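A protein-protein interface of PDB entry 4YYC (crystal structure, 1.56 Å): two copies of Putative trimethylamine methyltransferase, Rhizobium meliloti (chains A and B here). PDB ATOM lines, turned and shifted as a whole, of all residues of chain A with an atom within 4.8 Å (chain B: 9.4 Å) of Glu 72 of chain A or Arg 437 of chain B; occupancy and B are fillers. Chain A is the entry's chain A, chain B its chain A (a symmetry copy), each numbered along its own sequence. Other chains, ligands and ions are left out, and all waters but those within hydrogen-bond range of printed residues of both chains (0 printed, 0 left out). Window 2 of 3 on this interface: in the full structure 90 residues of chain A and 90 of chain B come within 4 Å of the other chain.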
ATOM      1  N   VAL A  68      -2.872  -6.963  -0.053  1.00  0.00           N
ATOM      2  CA  VAL A  68      -4.148  -6.887  -0.772  1.00  0.00           C
ATOM      3  C   VAL A  68      -5.264  -6.232   0.042  1.00  0.00           C
ATOM      4  O   VAL A  68      -5.942  -5.334  -0.414  1.00  0.00           O
ATOM      5  CB  VAL A  68      -4.601  -8.287  -1.230  1.00  0.00           C
ATOM      6  CG1 VAL A  68      -6.030  -8.247  -1.771  1.00  0.00           C
ATOM      7  CG2 VAL A  68      -3.641  -8.785  -2.305  1.00  0.00           C
ATOM      8  N   VAL A  69      -5.458  -6.683   1.263  1.00  0.00           N
ATOM      9  CA  VAL A  69      -6.461  -6.075   2.155  1.00  0.00           C
ATOM     10  C   VAL A  69      -6.216  -4.567   2.299  1.00  0.00           C
ATOM     11  O   VAL A  69      -7.152  -3.760   2.197  1.00  0.00           O
ATOM     12  CB  VAL A  69      -6.416  -6.763   3.532  1.00  0.00           C
ATOM     13  CG1 VAL A  69      -7.212  -5.980   4.579  1.00  0.00           C
ATOM     14  CG2 VAL A  69      -6.915  -8.206   3.415  1.00  0.00           C
ATOM     15  N   LEU A  70      -4.964  -4.195   2.555  1.00  0.00           N
ATOM     16  CA  LEU A  70      -4.628  -2.789   2.786  1.00  0.00           C
ATOM     17  C   LEU A  70      -4.916  -1.900   1.574  1.00  0.00           C
ATOM     18  O   LEU A  70      -5.261  -0.731   1.738  1.00  0.00           O
ATOM     19  CB  LEU A  70      -3.165  -2.624   3.185  1.00  0.00           C
ATOM     20  CG  LEU A  70      -2.831  -3.014   4.631  1.00  0.00           C
ATOM     21  CD1 LEU A  70      -1.323  -2.932   4.832  1.00  0.00           C
ATOM     22  CD2 LEU A  70      -3.535  -2.151   5.654  1.00  0.00           C
ATOM     23  N   GLU A  71      -4.705  -2.437   0.370  1.00  0.00           N
ATOM     24  CA  GLU A  71      -4.970  -1.667  -0.832  1.00  0.00           C
ATOM     25  C   GLU A  71      -6.463  -1.672  -1.211  1.00  0.00           C
ATOM     26  O   GLU A  71      -7.040  -0.618  -1.435  1.00  0.00           O
ATOM     27  CB  GLU A  71      -4.109  -2.136  -1.999  1.00  0.00           C
ATOM     28  CG  GLU A  71      -4.350  -1.260  -3.218  1.00  0.00           C
ATOM     29  CD  GLU A  71      -3.510  -1.591  -4.421  1.00  0.00           C
ATOM     30  OE1 GLU A  71      -2.772  -2.607  -4.440  1.00  0.00           O
ATOM     31  OE2 GLU A  71      -3.610  -0.793  -5.373  1.00  0.00           O
ATOM     32  N   GLU A  72      -7.067  -2.840  -1.308  1.00  0.00           N
ATOM     33  CA  GLU A  72      -8.446  -2.979  -1.787  1.00  0.00           C
ATOM     34  C   GLU A  72      -9.514  -2.584  -0.796  1.00  0.00           C
ATOM     35  O   GLU A  72     -10.505  -1.995  -1.167  1.00  0.00           O
ATOM     36  CB  GLU A  72      -8.728  -4.407  -2.235  1.00  0.00           C
ATOM     37  CG  GLU A  72      -7.900  -4.837  -3.418  1.00  0.00           C
ATOM     38  CD  GLU A  72      -8.233  -6.254  -3.885  1.00  0.00           C
ATOM     39  OE1 GLU A  72      -9.196  -6.897  -3.313  1.00  0.00           O
ATOM     40  OE2 GLU A  72      -7.494  -6.702  -4.786  1.00  0.00           O
ATOM     41  N   ILE A  73      -9.310  -2.921   0.461  1.00  0.00           N
ATOM     42  CA  ILE A  73     -10.331  -2.725   1.502  1.00  0.00           C
ATOM     43  C   ILE A  73      -9.990  -1.496   2.325  1.00  0.00           C
ATOM     44  O   ILE A  73     -10.856  -0.652   2.537  1.00  0.00           O
ATOM     45  CB  ILE A  73     -10.472  -3.970   2.406  1.00  0.00           C
ATOM     46  CG1 ILE A  73     -10.889  -5.162   1.539  1.00  0.00           C
ATOM     47  CG2 ILE A  73     -11.481  -3.696   3.509  1.00  0.00           C
ATOM     48  CD1 ILE A  73     -10.870  -6.486   2.265  1.00  0.00           C
ATOM     49  N   GLY A  74      -8.744  -1.385   2.759  1.00  0.00           N
ATOM     50  CA  GLY A  74      -8.299  -0.247   3.534  1.00  0.00           C
ATOM     51  C   GLY A  74      -8.605  -0.380   5.013  1.00  0.00           C
ATOM     52  O   GLY A  74      -9.171  -1.365   5.468  1.00  0.00           O
ATOM     53  N   HIS A 100      -6.724   3.726   1.946  1.00  0.00           N
ATOM     54  CA  HIS A 100      -6.264   2.653   1.071  1.00  0.00           C
ATOM     55  C   HIS A 100      -4.767   2.827   0.835  1.00  0.00           C
ATOM     56  O   HIS A 100      -4.304   3.908   0.449  1.00  0.00           O
ATOM     57  CB  HIS A 100      -7.036   2.671  -0.254  1.00  0.00           C
ATOM     58  CG  HIS A 100      -8.503   2.397  -0.093  1.00  0.00           C
ATOM     59  ND1 HIS A 100      -9.053   1.150  -0.313  1.00  0.00           N
ATOM     60  CD2 HIS A 100      -9.526   3.196   0.299  1.00  0.00           C
ATOM     61  CE1 HIS A 100     -10.353   1.199  -0.075  1.00  0.00           C
ATOM     62  NE2 HIS A 100     -10.669   2.434   0.279  1.00  0.00           N
ATOM     63  N   GLU B 428      -7.499 -21.871   0.203  1.00  0.00           N
ATOM     64  CA  GLU B 428      -8.139 -20.616  -0.218  1.00  0.00           C
ATOM     65  C   GLU B 428      -9.310 -20.265   0.709  1.00  0.00           C
ATOM     66  O   GLU B 428      -9.484 -19.099   1.120  1.00  0.00           O
ATOM     67  CB  GLU B 428      -8.572 -20.667  -1.721  1.00  0.00           C
ATOM     68  CG  GLU B 428      -7.458 -20.285  -2.650  1.00  0.00           C
ATOM     69  N   GLN B 431      -7.823 -18.906   3.922  1.00  0.00           N
ATOM     70  CA  GLN B 431      -7.316 -17.551   3.731  1.00  0.00           C
ATOM     71  C   GLN B 431      -8.391 -16.460   3.955  1.00  0.00           C
ATOM     72  O   GLN B 431      -8.079 -15.354   4.358  1.00  0.00           O
ATOM     73  CB  GLN B 431      -6.679 -17.403   2.367  1.00  0.00           C
ATOM     74  CG  GLN B 431      -5.361 -18.141   2.232  1.00  0.00           C
ATOM     75  CD  GLN B 431      -4.909 -18.232   0.779  1.00  0.00           C
ATOM     76  OE1 GLN B 431      -4.801 -17.219   0.095  1.00  0.00           O
ATOM     77  NE2 GLN B 431      -4.619 -19.438   0.316  1.00  0.00           N
ATOM     78  N   ALA B 432      -9.644 -16.794   3.655  1.00  0.00           N
ATOM     79  CA  ALA B 432     -10.794 -15.998   4.032  1.00  0.00           C
ATOM     80  C   ALA B 432     -10.850 -14.625   3.414  1.00  0.00           C
ATOM     81  O   ALA B 432     -11.425 -13.731   3.999  1.00  0.00           O
ATOM     82  CB  ALA B 432     -10.871 -15.891   5.570  1.00  0.00           C
ATOM     83  N   LEU B 433     -10.309 -14.445   2.198  1.00  0.00           N
ATOM     84  CA  LEU B 433     -10.259 -13.101   1.658  1.00  0.00           C
ATOM     85  C   LEU B 433     -11.635 -12.559   1.319  1.00  0.00           C
ATOM     86  O   LEU B 433     -11.892 -11.382   1.510  1.00  0.00           O
ATOM     87  CB  LEU B 433      -9.345 -13.030   0.441  1.00  0.00           C
ATOM     88  CG  LEU B 433      -7.860 -13.141   0.773  1.00  0.00           C
ATOM     89  CD1 LEU B 433      -7.002 -13.034  -0.494  1.00  0.00           C
ATOM     90  CD2 LEU B 433      -7.462 -12.072   1.781  1.00  0.00           C
ATOM     91  N   ASP B 434     -12.511 -13.419   0.810  1.00  0.00           N
ATOM     92  CA  ASP B 434     -13.880 -12.996   0.502  1.00  0.00           C
ATOM     93  C   ASP B 434     -14.672 -12.604   1.754  1.00  0.00           C
ATOM     94  O   ASP B 434     -15.456 -11.660   1.702  1.00  0.00           O
ATOM     95  CB  ASP B 434     -14.609 -14.090  -0.303  1.00  0.00           C
ATOM     96  CG  ASP B 434     -14.028 -14.255  -1.727  1.00  0.00           C
ATOM     97  OD1 ASP B 434     -13.558 -13.239  -2.315  1.00  0.00           O
ATOM     98  OD2 ASP B 434     -14.045 -15.399  -2.234  1.00  0.00           O
ATOM     99  N   ALA B 435     -14.446 -13.304   2.876  1.00  0.00           N
ATOM    100  CA  ALA B 435     -15.062 -12.939   4.156  1.00  0.00           C
ATOM    101  C   ALA B 435     -14.564 -11.584   4.639  1.00  0.00           C
ATOM    102  O   ALA B 435     -15.362 -10.740   5.029  1.00  0.00           O
ATOM    103  CB  ALA B 435     -14.799 -13.994   5.210  1.00  0.00           C
ATOM    104  N   ILE B 436     -13.258 -11.346   4.541  1.00  0.00           N
ATOM    105  CA  ILE B 436     -12.680 -10.034   4.928  1.00  0.00           C
ATOM    106  C   ILE B 436     -13.299  -8.894   4.066  1.00  0.00           C
ATOM    107  O   ILE B 436     -13.693  -7.840   4.578  1.00  0.00           O
ATOM    108  CB  ILE B 436     -11.133 -10.044   4.873  1.00  0.00           C
ATOM    109  CG1 ILE B 436     -10.565 -11.097   5.850  1.00  0.00           C
ATOM    110  CG2 ILE B 436     -10.581  -8.654   5.198  1.00  0.00           C
ATOM    111  CD1 ILE B 436      -9.072 -11.273   5.779  1.00  0.00           C
ATOM    112  N   ARG B 437     -13.431  -9.152   2.769  1.00  0.00           N
ATOM    113  CA  ARG B 437     -14.062  -8.186   1.859  1.00  0.00           C
ATOM    114  C   ARG B 437     -15.528  -7.916   2.165  1.00  0.00           C
ATOM    115  O   ARG B 437     -15.979  -6.761   2.147  1.00  0.00           O
ATOM    116  CB  ARG B 437     -14.000  -8.707   0.429  1.00  0.00           C
ATOM    117  CG  ARG B 437     -12.617  -8.794  -0.147  1.00  0.00           C
ATOM    118  CD  ARG B 437     -12.687  -9.291  -1.587  1.00  0.00           C
ATOM    119  NE  ARG B 437     -11.387  -9.117  -2.227  1.00  0.00           N
ATOM    120  CZ  ARG B 437     -10.522 -10.086  -2.512  1.00  0.00           C
ATOM    121  NH1 ARG B 437     -10.792 -11.389  -2.273  1.00  0.00           N
ATOM    122  NH2 ARG B 437      -9.365  -9.750  -3.089  1.00  0.00           N
ATOM    123  N   GLU B 438     -16.288  -8.984   2.383  1.00  0.00           N
ATOM    124  CA  GLU B 438     -17.743  -8.862   2.545  1.00  0.00           C
ATOM    125  C   GLU B 438     -18.082  -8.221   3.890  1.00  0.00           C
ATOM    126  O   GLU B 438     -19.005  -7.425   3.987  1.00  0.00           O
ATOM    127  CB  GLU B 438     -18.428 -10.233   2.412  1.00  0.00           C
ATOM    128  N   VAL B 439     -17.311  -8.528   4.919  1.00  0.00           N
ATOM    129  CA  VAL B 439     -17.548  -7.937   6.235  1.00  0.00           C
ATOM    130  C   VAL B 439     -17.029  -6.507   6.209  1.00  0.00           C
ATOM    131  O   VAL B 439     -17.785  -5.548   6.454  1.00  0.00           O
ATOM    132  CB  VAL B 439     -16.890  -8.794   7.348  1.00  0.00           C
ATOM    133  CG1 VAL B 439     -16.911  -8.115   8.712  1.00  0.00           C
ATOM    134  CG2 VAL B 439     -17.631 -10.114   7.438  1.00  0.00           C
ATOM    135  N   GLY B 440     -15.732  -6.379   5.929  1.00  0.00           N
ATOM    136  CA  GLY B 440     -15.076  -5.070   5.842  1.00  0.00           C
ATOM    137  C   GLY B 440     -14.901  -4.370   7.195  1.00  0.00           C
ATOM    138  O   GLY B 440     -15.305  -4.882   8.261  1.00  0.00           O
ATOM    139  N   PRO B 441     -14.283  -3.187   7.169  1.00  0.00           N
ATOM    140  CA  PRO B 441     -13.990  -2.517   8.438  1.00  0.00           C
ATOM    141  C   PRO B 441     -15.240  -2.141   9.231  1.00  0.00           C
ATOM    142  O   PRO B 441     -16.223  -1.682   8.662  1.00  0.00           O
ATOM    143  CB  PRO B 441     -13.225  -1.256   7.990  1.00  0.00           C
ATOM    144  CG  PRO B 441     -12.612  -1.630   6.671  1.00  0.00           C
ATOM    145  CD  PRO B 441     -13.684  -2.469   6.022  1.00  0.00           C
ATOM    146  N   SER B 443     -17.401  -3.921  10.849  1.00  0.00           N
ATOM    147  CA  SER B 443     -18.495  -4.872  10.939  1.00  0.00           C
ATOM    148  C   SER B 443     -18.081  -6.060  11.825  1.00  0.00           C
ATOM    149  O   SER B 443     -17.266  -5.923  12.733  1.00  0.00           O
ATOM    150  CB  SER B 443     -18.965  -5.228   9.522  1.00  0.00           C
ATOM    151  OG  SER B 443     -20.155  -5.991   9.574  1.00  0.00           O
ATOM    152  N   TYR B 445     -18.021 -10.715  11.954  1.00  0.00           N
ATOM    153  CA  TYR B 445     -18.028 -11.938  11.182  1.00  0.00           C
ATOM    154  C   TYR B 445     -19.011 -13.025  11.669  1.00  0.00           C
ATOM    155  O   TYR B 445     -19.057 -14.108  11.051  1.00  0.00           O
ATOM    156  CB  TYR B 445     -16.633 -12.548  11.204  1.00  0.00           C
ATOM    157  CG  TYR B 445     -15.582 -11.746  10.462  1.00  0.00           C
ATOM    158  CD1 TYR B 445     -14.923 -10.695  11.068  1.00  0.00           C
ATOM    159  CD2 TYR B 445     -15.201 -12.109   9.171  1.00  0.00           C
ATOM    160  CE1 TYR B 445     -13.924  -9.978  10.397  1.00  0.00           C
ATOM    161  CE2 TYR B 445     -14.218 -11.405   8.485  1.00  0.00           C
ATOM    162  CZ  TYR B 445     -13.586 -10.340   9.097  1.00  0.00           C
ATOM    163  OH  TYR B 445     -12.601  -9.663   8.422  1.00  0.00           O
ATOM    164  N   CYS B 448     -21.663 -14.339   8.980  1.00  0.00           N
ATOM    165  CA  CYS B 448     -21.323 -14.815   7.636  1.00  0.00           C
ATOM    166  C   CYS B 448     -21.077 -16.340   7.526  1.00  0.00           C
ATOM    167  O   CYS B 448     -20.777 -17.043   8.503  1.00  0.00           O
ATOM    168  CB  CYS B 448     -20.214 -13.970   6.980  1.00  0.00           C
ATOM    169  SG  CYS B 448     -18.598 -14.043   7.747  1.00  0.00           S
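N of Gly 74 of chain A sits at hydrogen-bond distance from O of Val 69 of chain A, at 2.9 Å. OD1 of Asp 434 of chain B is in salt-bridge range of NH1 of Arg 437 of chain B, 3.3 Å away.
The side-chain carboxylate (OE1) of Glu 72 of chain A is in salt-bridge range of the guanidinium group (NH2) of Arg 437 of chain B, at 2.9 Å.
Leu 70 of chain A touches none of the printed residues of chain B. Of chain B, only Arg 437 comes within 4 Å of Glu 72 of chain A. Of chain B, only Ile 436 (3.7 Å), Arg 437 (3.6 Å) and Pro 441 (3.6 Å) come within 4 Å of Ile 73 of chain A. Of the printed residues of chain B, Gly 74 of chain A touches Pro 441. Printed residues of chain A within 4 Å of Ile 436 of chain B: Ile 73. Of chain A, only Val 68 (3.9 Å), Glu 72 (2.9 Å) and Ile 73 (3.6 Å) come within 4 Å of Arg 437 of chain B. Glu 438 of chain B touches none of the printed residues of chain A.
Of the 8 printed residues of chain A, 4 touch a printed residue of chain B. Printed residues of chain A that touch a printed residue of chain B: Val 68, Glu 72, Ile 73 and Gly 74. Along chain A the printed residues that touch a printed residue of chain B span positions 68 to 74. Hydrophobic or aromatic side chains of chain B within 4 Å of the printed part of chain A: Ile 436 and Pro 441. Among the printed residues, 6 pairs touch across the chains.
Among the printed residues, pairs that only touch across the chains: Ile 73 of chain A with Pro 441 of chain B (3.6 Å), Ile 73 of chain A with Arg 437 of chain B (3.6 Å), Gly 74 of chain A with Pro 441 of chain B (3.7 Å), Ile 73 of chain A with Ile 436 of chain B (3.7 Å) and Val 68 of chain A with Arg 437 of chain B (3.9 Å).
No position is printed for both chains.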
